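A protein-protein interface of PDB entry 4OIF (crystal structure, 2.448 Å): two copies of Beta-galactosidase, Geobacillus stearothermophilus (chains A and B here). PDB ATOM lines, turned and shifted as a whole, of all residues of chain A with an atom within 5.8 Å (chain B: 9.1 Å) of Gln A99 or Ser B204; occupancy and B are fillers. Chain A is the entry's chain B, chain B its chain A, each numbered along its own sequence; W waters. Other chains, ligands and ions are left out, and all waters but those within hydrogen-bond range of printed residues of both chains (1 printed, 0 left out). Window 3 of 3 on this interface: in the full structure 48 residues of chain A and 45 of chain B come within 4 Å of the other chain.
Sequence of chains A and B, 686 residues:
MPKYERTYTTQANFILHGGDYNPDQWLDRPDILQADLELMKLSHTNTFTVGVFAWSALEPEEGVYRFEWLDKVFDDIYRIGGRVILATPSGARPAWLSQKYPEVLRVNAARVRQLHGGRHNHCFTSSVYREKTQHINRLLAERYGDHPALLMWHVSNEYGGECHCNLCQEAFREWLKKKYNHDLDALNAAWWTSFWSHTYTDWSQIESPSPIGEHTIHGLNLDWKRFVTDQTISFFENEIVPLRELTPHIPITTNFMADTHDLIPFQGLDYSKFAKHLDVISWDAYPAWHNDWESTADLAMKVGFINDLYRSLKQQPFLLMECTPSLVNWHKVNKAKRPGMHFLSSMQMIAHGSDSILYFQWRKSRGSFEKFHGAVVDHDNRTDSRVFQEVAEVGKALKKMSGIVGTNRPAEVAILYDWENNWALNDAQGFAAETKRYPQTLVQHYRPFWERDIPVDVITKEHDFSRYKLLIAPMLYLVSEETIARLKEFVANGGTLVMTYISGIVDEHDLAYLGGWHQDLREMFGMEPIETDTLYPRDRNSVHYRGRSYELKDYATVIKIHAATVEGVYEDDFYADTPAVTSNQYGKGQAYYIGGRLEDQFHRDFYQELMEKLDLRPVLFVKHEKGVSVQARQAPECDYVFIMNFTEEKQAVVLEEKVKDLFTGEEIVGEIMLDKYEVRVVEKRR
Water W1 bridges the side-chain hydroxyl of Thr B201 (2.7 Å) and the backbone NH of Trp A96 (3.3 Å).
Of the printed residues of chain B, Ala A95 touches Gln B205 (3.6 Å). Of the printed residues of chain B, Trp A96 touches Thr B201 and Gln B205. No residue of chain B comes within 4 Å of Ser A98. Gln A99 touches just these residues of chain B: Ser B204 (2.7 Å) and Gln B205 (3.5 Å). Of the printed residues of chain A, Thr B201 touches Trp A96. Ser B204 touches just one residue of chain A: Gln A99 (2.7 Å). Of the printed residues of chain A, Gln B205 touches Ala A95 (3.6 Å), Trp A96 (3.5 Å) and Gln A99 (3.5 Å). Ile B206 touches none of the printed residues of chain A. Glu B207 touches none of the printed residues of chain A. The nearest residue of chain B that does not touch Gln A99 is Asp B202 (5.1 Å).
Among the printed residues, merely in contact across the chains: Trp A96 with Gln B205 (3.5 Å), Gln A99 with Gln B205 (3.5 Å), Ala A95 with Gln B205 (3.6 Å) and Trp A96 with Thr B201 (3.9 Å).
Hydrophobic or aromatic side chains of chain A within 4 Å of the printed part of chain B: Ala A95 and Trp A96. Along chain A the printed residues that touch a printed residue of chain B span positions 95 to 99. Of the 16 printed residues of chain B, 3 touch a printed residue of chain A. Among the printed residues, 5 pairs touch across the chains. Among the printed residues, no Asp or Glu carboxylate lies within 4 Å of a Lys or Arg side-chain nitrogen of the other chain.
No position is printed for both chains.
The side-chain amide oxygen of Gln B205 is in hydrogen-bond range of the backbone NH of Thr B201, 2.8 Å away. The side-chain amide oxygen (OE1) of Gln B205 sits at hydrogen-bond distance from the backbone NH (N) of Asp B202 (3.3 Å). The side-chain hydroxyl of Ser B204 is in hydrogen-bond range of the side-chain carboxylate of Asp B202 (2.7 Å).
The side-chain hydroxyl (OG) of Ser B204 lies within hydrogen-bond range of the side-chain amide nitrogen (NE2) of Gln A99 (2.7 Å).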
ATOM      1  N   PRO A  94      18.118 -34.980  19.815  1.00  0.00           N
ATOM      2  CA  PRO A  94      16.880 -34.271  19.454  1.00  0.00           C
ATOM      3  C   PRO A  94      17.162 -32.821  19.048  1.00  0.00           C
ATOM      4  O   PRO A  94      18.194 -32.242  19.431  1.00  0.00           O
ATOM      5  CB  PRO A  94      16.040 -34.328  20.738  1.00  0.00           C
ATOM      6  CG  PRO A  94      16.554 -35.507  21.481  1.00  0.00           C
ATOM      7  CD  PRO A  94      18.042 -35.564  21.162  1.00  0.00           C
ATOM      8  N   ALA A  95      16.265 -32.252  18.251  1.00  0.00           N
ATOM      9  CA  ALA A  95      16.380 -30.850  17.865  1.00  0.00           C
ATOM     10  C   ALA A  95      16.476 -29.926  19.091  1.00  0.00           C
ATOM     11  O   ALA A  95      17.308 -29.009  19.107  1.00  0.00           O
ATOM     12  CB  ALA A  95      15.200 -30.447  16.979  1.00  0.00           C
ATOM     13  N   TRP A  96      15.660 -30.183  20.121  1.00  0.00           N
ATOM     14  CA  TRP A  96      15.633 -29.308  21.288  1.00  0.00           C
ATOM     15  C   TRP A  96      17.001 -29.256  21.918  1.00  0.00           C
ATOM     16  O   TRP A  96      17.402 -28.226  22.463  1.00  0.00           O
ATOM     17  CB  TRP A  96      14.566 -29.730  22.331  1.00  0.00           C
ATOM     18  CG  TRP A  96      14.660 -31.120  22.977  1.00  0.00           C
ATOM     19  CD1 TRP A  96      13.863 -32.207  22.709  1.00  0.00           C
ATOM     20  CD2 TRP A  96      15.557 -31.538  24.026  1.00  0.00           C
ATOM     21  NE1 TRP A  96      14.219 -33.270  23.506  1.00  0.00           N
ATOM     22  CE2 TRP A  96      15.256 -32.887  24.323  1.00  0.00           C
ATOM     23  CE3 TRP A  96      16.594 -30.909  24.730  1.00  0.00           C
ATOM     24  CZ2 TRP A  96      15.962 -33.616  25.287  1.00  0.00           C
ATOM     25  CZ3 TRP A  96      17.291 -31.634  25.682  1.00  0.00           C
ATOM     26  CH2 TRP A  96      16.977 -32.971  25.952  1.00  0.00           C
ATOM     27  N   LEU A  97      17.733 -30.358  21.806  1.00  0.00           N
ATOM     28  CA  LEU A  97      19.015 -30.459  22.471  1.00  0.00           C
ATOM     29  C   LEU A  97      20.044 -29.598  21.737  1.00  0.00           C
ATOM     30  O   LEU A  97      20.793 -28.855  22.365  1.00  0.00           O
ATOM     31  CB  LEU A  97      19.456 -31.916  22.558  1.00  0.00           C
ATOM     32  CG  LEU A  97      20.424 -32.282  23.685  1.00  0.00           C
ATOM     33  CD1 LEU A  97      20.202 -33.736  24.111  1.00  0.00           C
ATOM     34  CD2 LEU A  97      21.862 -32.062  23.279  1.00  0.00           C
ATOM     35  N   SER A  98      20.064 -29.672  20.411  1.00  0.00           N
ATOM     36  CA  SER A  98      20.950 -28.817  19.624  1.00  0.00           C
ATOM     37  C   SER A  98      20.621 -27.355  19.837  1.00  0.00           C
ATOM     38  O   SER A  98      21.511 -26.513  19.955  1.00  0.00           O
ATOM     39  CB  SER A  98      20.856 -29.136  18.130  1.00  0.00           C
ATOM     40  OG  SER A  98      21.143 -30.487  17.869  1.00  0.00           O
ATOM     41  N   GLN A  99      19.332 -27.046  19.861  1.00  0.00           N
ATOM     42  CA  GLN A  99      18.917 -25.666  20.046  1.00  0.00           C
ATOM     43  C   GLN A  99      19.380 -25.128  21.412  1.00  0.00           C
ATOM     44  O   GLN A  99      19.908 -24.022  21.508  1.00  0.00           O
ATOM     45  CB  GLN A  99      17.399 -25.547  19.897  1.00  0.00           C
ATOM     46  CG  GLN A  99      16.908 -24.115  19.739  1.00  0.00           C
ATOM     47  CD  GLN A  99      15.385 -24.011  19.751  1.00  0.00           C
ATOM     48  OE1 GLN A  99      14.714 -24.667  20.551  1.00  0.00           O
ATOM     49  NE2 GLN A  99      14.836 -23.202  18.851  1.00  0.00           N
ATOM     50  N   LYS A 100      19.205 -25.908  22.470  1.00  0.00           N
ATOM     51  CA  LYS A 100      19.572 -25.410  23.793  1.00  0.00           C
ATOM     52  C   LYS A 100      21.064 -25.574  24.097  1.00  0.00           C
ATOM     53  O   LYS A 100      21.637 -24.827  24.898  1.00  0.00           O
ATOM     54  CB  LYS A 100      18.754 -26.102  24.872  1.00  0.00           C
ATOM     55  CG  LYS A 100      18.953 -25.491  26.235  1.00  0.00           C
ATOM     56  CD  LYS A 100      18.019 -26.100  27.242  1.00  0.00           C
ATOM     57  CE  LYS A 100      18.259 -25.530  28.617  1.00  0.00           C
ATOM     58  NZ  LYS A 100      17.394 -26.200  29.628  1.00  0.00           N
ATOM     59  N   TYR A 101      21.705 -26.542  23.458  1.00  0.00           N
ATOM     60  CA  TYR A 101      23.107 -26.788  23.751  1.00  0.00           C
ATOM     61  C   TYR A 101      23.940 -26.832  22.475  1.00  0.00           C
ATOM     62  O   TYR A 101      24.424 -27.887  22.083  1.00  0.00           O
ATOM     63  CB  TYR A 101      23.254 -28.086  24.551  1.00  0.00           C
ATOM     64  CG  TYR A 101      22.464 -28.093  25.840  1.00  0.00           C
ATOM     65  CD1 TYR A 101      22.979 -27.525  26.998  1.00  0.00           C
ATOM     66  CD2 TYR A 101      21.201 -28.658  25.899  1.00  0.00           C
ATOM     67  CE1 TYR A 101      22.254 -27.528  28.183  1.00  0.00           C
ATOM     68  CE2 TYR A 101      20.468 -28.660  27.069  1.00  0.00           C
ATOM     69  CZ  TYR A 101      21.001 -28.098  28.213  1.00  0.00           C
ATOM     70  OH  TYR A 101      20.271 -28.108  29.381  1.00  0.00           O
ATOM     71  N   PRO A 102      24.138 -25.669  21.842  1.00  0.00           N
ATOM     72  CA  PRO A 102      24.853 -25.575  20.557  1.00  0.00           C
ATOM     73  C   PRO A 102      26.231 -26.230  20.590  1.00  0.00           C
ATOM     74  O   PRO A 102      26.734 -26.645  19.547  1.00  0.00           O
ATOM     75  CB  PRO A 102      24.996 -24.063  20.332  1.00  0.00           C
ATOM     76  CG  PRO A 102      23.980 -23.427  21.239  1.00  0.00           C
ATOM     77  CD  PRO A 102      23.802 -24.347  22.400  1.00  0.00           C
ATOM     78  N   GLN B 169      14.401 -17.198   7.015  1.00  0.00           N
ATOM     79  CA  GLN B 169      14.105 -18.308   7.918  1.00  0.00           C
ATOM     80  C   GLN B 169      12.772 -18.046   8.593  1.00  0.00           C
ATOM     81  O   GLN B 169      11.917 -18.951   8.715  1.00  0.00           O
ATOM     82  CB  GLN B 169      15.202 -18.484   8.978  1.00  0.00           C
ATOM     83  CG  GLN B 169      16.591 -18.780   8.415  1.00  0.00           C
ATOM     84  CD  GLN B 169      16.680 -20.130   7.750  1.00  0.00           C
ATOM     85  OE1 GLN B 169      15.942 -21.051   8.092  1.00  0.00           O
ATOM     86  NE2 GLN B 169      17.586 -20.260   6.789  1.00  0.00           N
ATOM     87  N   GLU B 170      12.596 -16.803   9.041  1.00  0.00           N
ATOM     88  CA  GLU B 170      11.348 -16.461   9.701  1.00  0.00           C
ATOM     89  C   GLU B 170      10.179 -16.542   8.726  1.00  0.00           C
ATOM     90  O   GLU B 170       9.122 -17.092   9.064  1.00  0.00           O
ATOM     91  CB  GLU B 170      11.430 -15.083  10.353  1.00  0.00           C
ATOM     92  CG  GLU B 170      11.725 -15.160  11.852  1.00  0.00           C
ATOM     93  CD  GLU B 170      10.768 -16.109  12.595  1.00  0.00           C
ATOM     94  OE1 GLU B 170       9.554 -16.120  12.269  1.00  0.00           O
ATOM     95  OE2 GLU B 170      11.227 -16.851  13.498  1.00  0.00           O
ATOM     96  N   ARG B 173       9.272 -20.120   8.209  1.00  0.00           N
ATOM     97  CA  ARG B 173       8.500 -20.579   9.360  1.00  0.00           C
ATOM     98  C   ARG B 173       7.042 -20.135   9.294  1.00  0.00           C
ATOM     99  O   ARG B 173       6.140 -20.941   9.546  1.00  0.00           O
ATOM    100  CB  ARG B 173       9.131 -20.097  10.652  1.00  0.00           C
ATOM    101  CG  ARG B 173      10.242 -20.994  11.119  1.00  0.00           C
ATOM    102  CD  ARG B 173      10.886 -20.483  12.387  1.00  0.00           C
ATOM    103  NE  ARG B 173      12.269 -20.922  12.423  1.00  0.00           N
ATOM    104  CZ  ARG B 173      13.306 -20.106  12.308  1.00  0.00           C
ATOM    105  NH1 ARG B 173      13.112 -18.797  12.203  1.00  0.00           N
ATOM    106  NH2 ARG B 173      14.537 -20.599  12.324  1.00  0.00           N
ATOM    107  N   GLU B 174       6.805 -18.872   8.944  1.00  0.00           N
ATOM    108  CA  GLU B 174       5.427 -18.387   8.834  1.00  0.00           C
ATOM    109  C   GLU B 174       4.680 -19.094   7.708  1.00  0.00           C
ATOM    110  O   GLU B 174       3.491 -19.432   7.836  1.00  0.00           O
ATOM    111  CB  GLU B 174       5.401 -16.871   8.632  1.00  0.00           C
ATOM    112  CG  GLU B 174       5.817 -16.097   9.883  1.00  0.00           C
ATOM    113  CD  GLU B 174       4.961 -16.463  11.092  1.00  0.00           C
ATOM    114  OE1 GLU B 174       3.713 -16.456  10.946  1.00  0.00           O
ATOM    115  OE2 GLU B 174       5.535 -16.777  12.170  1.00  0.00           O
ATOM    116  N   LEU B 176       5.270 -22.130   6.723  1.00  0.00           N
ATOM    117  CA  LEU B 176       4.998 -23.490   7.159  1.00  0.00           C
ATOM    118  C   LEU B 176       3.823 -23.512   8.135  1.00  0.00           C
ATOM    119  O   LEU B 176       3.011 -24.443   8.120  1.00  0.00           O
ATOM    120  CB  LEU B 176       6.252 -24.115   7.789  1.00  0.00           C
ATOM    121  CG  LEU B 176       7.339 -24.639   6.830  1.00  0.00           C
ATOM    122  CD1 LEU B 176       8.573 -25.032   7.612  1.00  0.00           C
ATOM    123  CD2 LEU B 176       6.855 -25.821   5.988  1.00  0.00           C
ATOM    124  N   LYS B 177       3.731 -22.494   8.987  1.00  0.00           N
ATOM    125  CA  LYS B 177       2.600 -22.405   9.899  1.00  0.00           C
ATOM    126  C   LYS B 177       1.294 -22.266   9.114  1.00  0.00           C
ATOM    127  O   LYS B 177       0.313 -22.944   9.431  1.00  0.00           O
ATOM    128  CB  LYS B 177       2.766 -21.243  10.876  1.00  0.00           C
ATOM    129  CG  LYS B 177       3.867 -21.460  11.888  1.00  0.00           C
ATOM    130  CD  LYS B 177       3.998 -20.241  12.748  1.00  0.00           C
ATOM    131  CE  LYS B 177       5.139 -20.367  13.727  1.00  0.00           C
ATOM    132  NZ  LYS B 177       5.404 -19.057  14.377  1.00  0.00           N
ATOM    133  N   LEU B 184       2.083 -28.571  14.405  1.00  0.00           N
ATOM    134  CA  LEU B 184       3.415 -29.170  14.343  1.00  0.00           C
ATOM    135  C   LEU B 184       3.348 -30.697  14.218  1.00  0.00           C
ATOM    136  O   LEU B 184       4.213 -31.304  13.595  1.00  0.00           O
ATOM    137  CB  LEU B 184       4.222 -28.753  15.569  1.00  0.00           C
ATOM    138  CG  LEU B 184       5.734 -28.575  15.470  1.00  0.00           C
ATOM    139  CD1 LEU B 184       6.130 -27.748  14.268  1.00  0.00           C
ATOM    140  CD2 LEU B 184       6.227 -27.909  16.739  1.00  0.00           C
ATOM    141  N   TYR B 200      10.410 -32.204  15.376  1.00  0.00           N
ATOM    142  CA  TYR B 200      10.501 -30.823  15.832  1.00  0.00           C
ATOM    143  C   TYR B 200       9.509 -30.580  16.951  1.00  0.00           C
ATOM    144  O   TYR B 200       8.344 -30.948  16.837  1.00  0.00           O
ATOM    145  CB  TYR B 200      10.241 -29.854  14.679  1.00  0.00           C
ATOM    146  CG  TYR B 200      11.244 -29.940  13.556  1.00  0.00           C
ATOM    147  CD1 TYR B 200      12.532 -29.420  13.697  1.00  0.00           C
ATOM    148  CD2 TYR B 200      10.911 -30.542  12.348  1.00  0.00           C
ATOM    149  CE1 TYR B 200      13.460 -29.487  12.658  1.00  0.00           C
ATOM    150  CE2 TYR B 200      11.828 -30.611  11.307  1.00  0.00           C
ATOM    151  CZ  TYR B 200      13.096 -30.081  11.467  1.00  0.00           C
ATOM    152  OH  TYR B 200      14.004 -30.159  10.433  1.00  0.00           O
ATOM    153  N   THR B 201       9.959 -29.949  18.027  1.00  0.00           N
ATOM    154  CA  THR B 201       9.075 -29.695  19.158  1.00  0.00           C
ATOM    155  C   THR B 201       8.796 -28.205  19.342  1.00  0.00           C
ATOM    156  O   THR B 201       8.093 -27.808  20.266  1.00  0.00           O
ATOM    157  CB  THR B 201       9.647 -30.298  20.462  1.00  0.00           C
ATOM    158  OG1 THR B 201      11.051 -30.024  20.557  1.00  0.00           O
ATOM    159  CG2 THR B 201       9.433 -31.802  20.475  1.00  0.00           C
ATOM    160  N   ASP B 202       9.331 -27.382  18.447  1.00  0.00           N
ATOM    161  CA  ASP B 202       9.006 -25.956  18.426  1.00  0.00           C
ATOM    162  C   ASP B 202       9.324 -25.403  17.050  1.00  0.00           C
ATOM    163  O   ASP B 202      10.357 -25.748  16.470  1.00  0.00           O
ATOM    164  CB  ASP B 202       9.789 -25.185  19.499  1.00  0.00           C
ATOM    165  CG  ASP B 202       9.277 -23.757  19.693  1.00  0.00           C
ATOM    166  OD1 ASP B 202       9.708 -22.834  18.959  1.00  0.00           O
ATOM    167  OD2 ASP B 202       8.434 -23.563  20.591  1.00  0.00           O
ATOM    168  N   TRP B 203       8.448 -24.542  16.538  1.00  0.00           N
ATOM    169  CA  TRP B 203       8.623 -23.938  15.219  1.00  0.00           C
ATOM    170  C   TRP B 203       9.962 -23.221  15.042  1.00  0.00           C
ATOM    171  O   TRP B 203      10.475 -23.132  13.935  1.00  0.00           O
ATOM    172  CB  TRP B 203       7.497 -22.947  14.935  1.00  0.00           C
ATOM    173  CG  TRP B 203       6.166 -23.579  14.798  1.00  0.00           C
ATOM    174  CD1 TRP B 203       5.195 -23.662  15.755  1.00  0.00           C
ATOM    175  CD2 TRP B 203       5.645 -24.237  13.637  1.00  0.00           C
ATOM    176  NE1 TRP B 203       4.097 -24.321  15.256  1.00  0.00           N
ATOM    177  CE2 TRP B 203       4.345 -24.686  13.961  1.00  0.00           C
ATOM    178  CE3 TRP B 203       6.147 -24.488  12.358  1.00  0.00           C
ATOM    179  CZ2 TRP B 203       3.542 -25.372  13.051  1.00  0.00           C
ATOM    180  CZ3 TRP B 203       5.345 -25.174  11.450  1.00  0.00           C
ATOM    181  CH2 TRP B 203       4.060 -25.604  11.802  1.00  0.00           C
ATOM    182  N   SER B 204      10.520 -22.706  16.130  1.00  0.00           N
ATOM    183  CA  SER B 204      11.807 -22.031  16.069  1.00  0.00           C
ATOM    184  C   SER B 204      12.952 -22.972  15.700  1.00  0.00           C
ATOM    185  O   SER B 204      14.032 -22.517  15.342  1.00  0.00           O
ATOM    186  CB  SER B 204      12.120 -21.366  17.408  1.00  0.00           C
ATOM    187  OG  SER B 204      12.282 -22.337  18.425  1.00  0.00           O
ATOM    188  N   GLN B 205      12.726 -24.277  15.799  1.00  0.00           N
ATOM    189  CA  GLN B 205      13.788 -25.233  15.498  1.00  0.00           C
ATOM    190  C   GLN B 205      13.929 -25.459  14.005  1.00  0.00           C
ATOM    191  O   GLN B 205      15.006 -25.769  13.522  1.00  0.00           O
ATOM    192  CB  GLN B 205      13.539 -26.569  16.197  1.00  0.00           C
ATOM    193  CG  GLN B 205      13.736 -26.543  17.705  1.00  0.00           C
ATOM    194  CD  GLN B 205      12.949 -27.636  18.386  1.00  0.00           C
ATOM    195  OE1 GLN B 205      12.327 -28.467  17.722  1.00  0.00           O
ATOM    196  NE2 GLN B 205      12.958 -27.641  19.712  1.00  0.00           N
ATOM    197  N   ILE B 206      12.840 -25.297  13.271  1.00  0.00           N
ATOM    198  CA  ILE B 206      12.864 -25.553  11.842  1.00  0.00           C
ATOM    199  C   ILE B 206      13.642 -24.488  11.065  1.00  0.00           C
ATOM    200  O   ILE B 206      13.310 -23.311  11.116  1.00  0.00           O
ATOM    201  CB  ILE B 206      11.439 -25.635  11.283  1.00  0.00           C
ATOM    202  CG1 ILE B 206      10.675 -26.751  12.001  1.00  0.00           C
ATOM    203  CG2 ILE B 206      11.484 -25.844   9.775  1.00  0.00           C
ATOM    204  CD1 ILE B 206       9.174 -26.750  11.762  1.00  0.00           C
ATOM    205  N   GLU B 207      14.697 -24.894  10.372  1.00  0.00           N
ATOM    206  CA  GLU B 207      15.409 -23.986   9.482  1.00  0.00           C
ATOM    207  C   GLU B 207      15.486 -24.600   8.089  1.00  0.00           C
ATOM    208  O   GLU B 207      15.239 -25.793   7.916  1.00  0.00           O
ATOM    209  CB  GLU B 207      16.811 -23.645  10.028  1.00  0.00           C
ATOM    210  CG  GLU B 207      17.482 -24.730  10.879  1.00  0.00           C
ATOM    211  CD  GLU B 207      18.578 -24.183  11.810  1.00  0.00           C
ATOM    212  OE1 GLU B 207      19.469 -24.959  12.220  1.00  0.00           O
ATOM    213  OE2 GLU B 207      18.539 -22.980  12.141  1.00  0.00           O
ATOM    214  N   SER B 208      15.814 -23.779   7.104  1.00  0.00           N
ATOM    215  CA  SER B 208      15.951 -24.253   5.731  1.00  0.00           C
ATOM    216  C   SER B 208      17.033 -25.327   5.645  1.00  0.00           C
ATOM    217  O   SER B 208      17.949 -25.354   6.468  1.00  0.00           O
ATOM    218  CB  SER B 208      16.289 -23.098   4.805  1.00  0.00           C
ATOM    219  OG  SER B 208      17.547 -22.561   5.159  1.00  0.00           O
HETATM  220  O   HOH W   1      12.855 -31.750  19.561  1.00  0.00           O
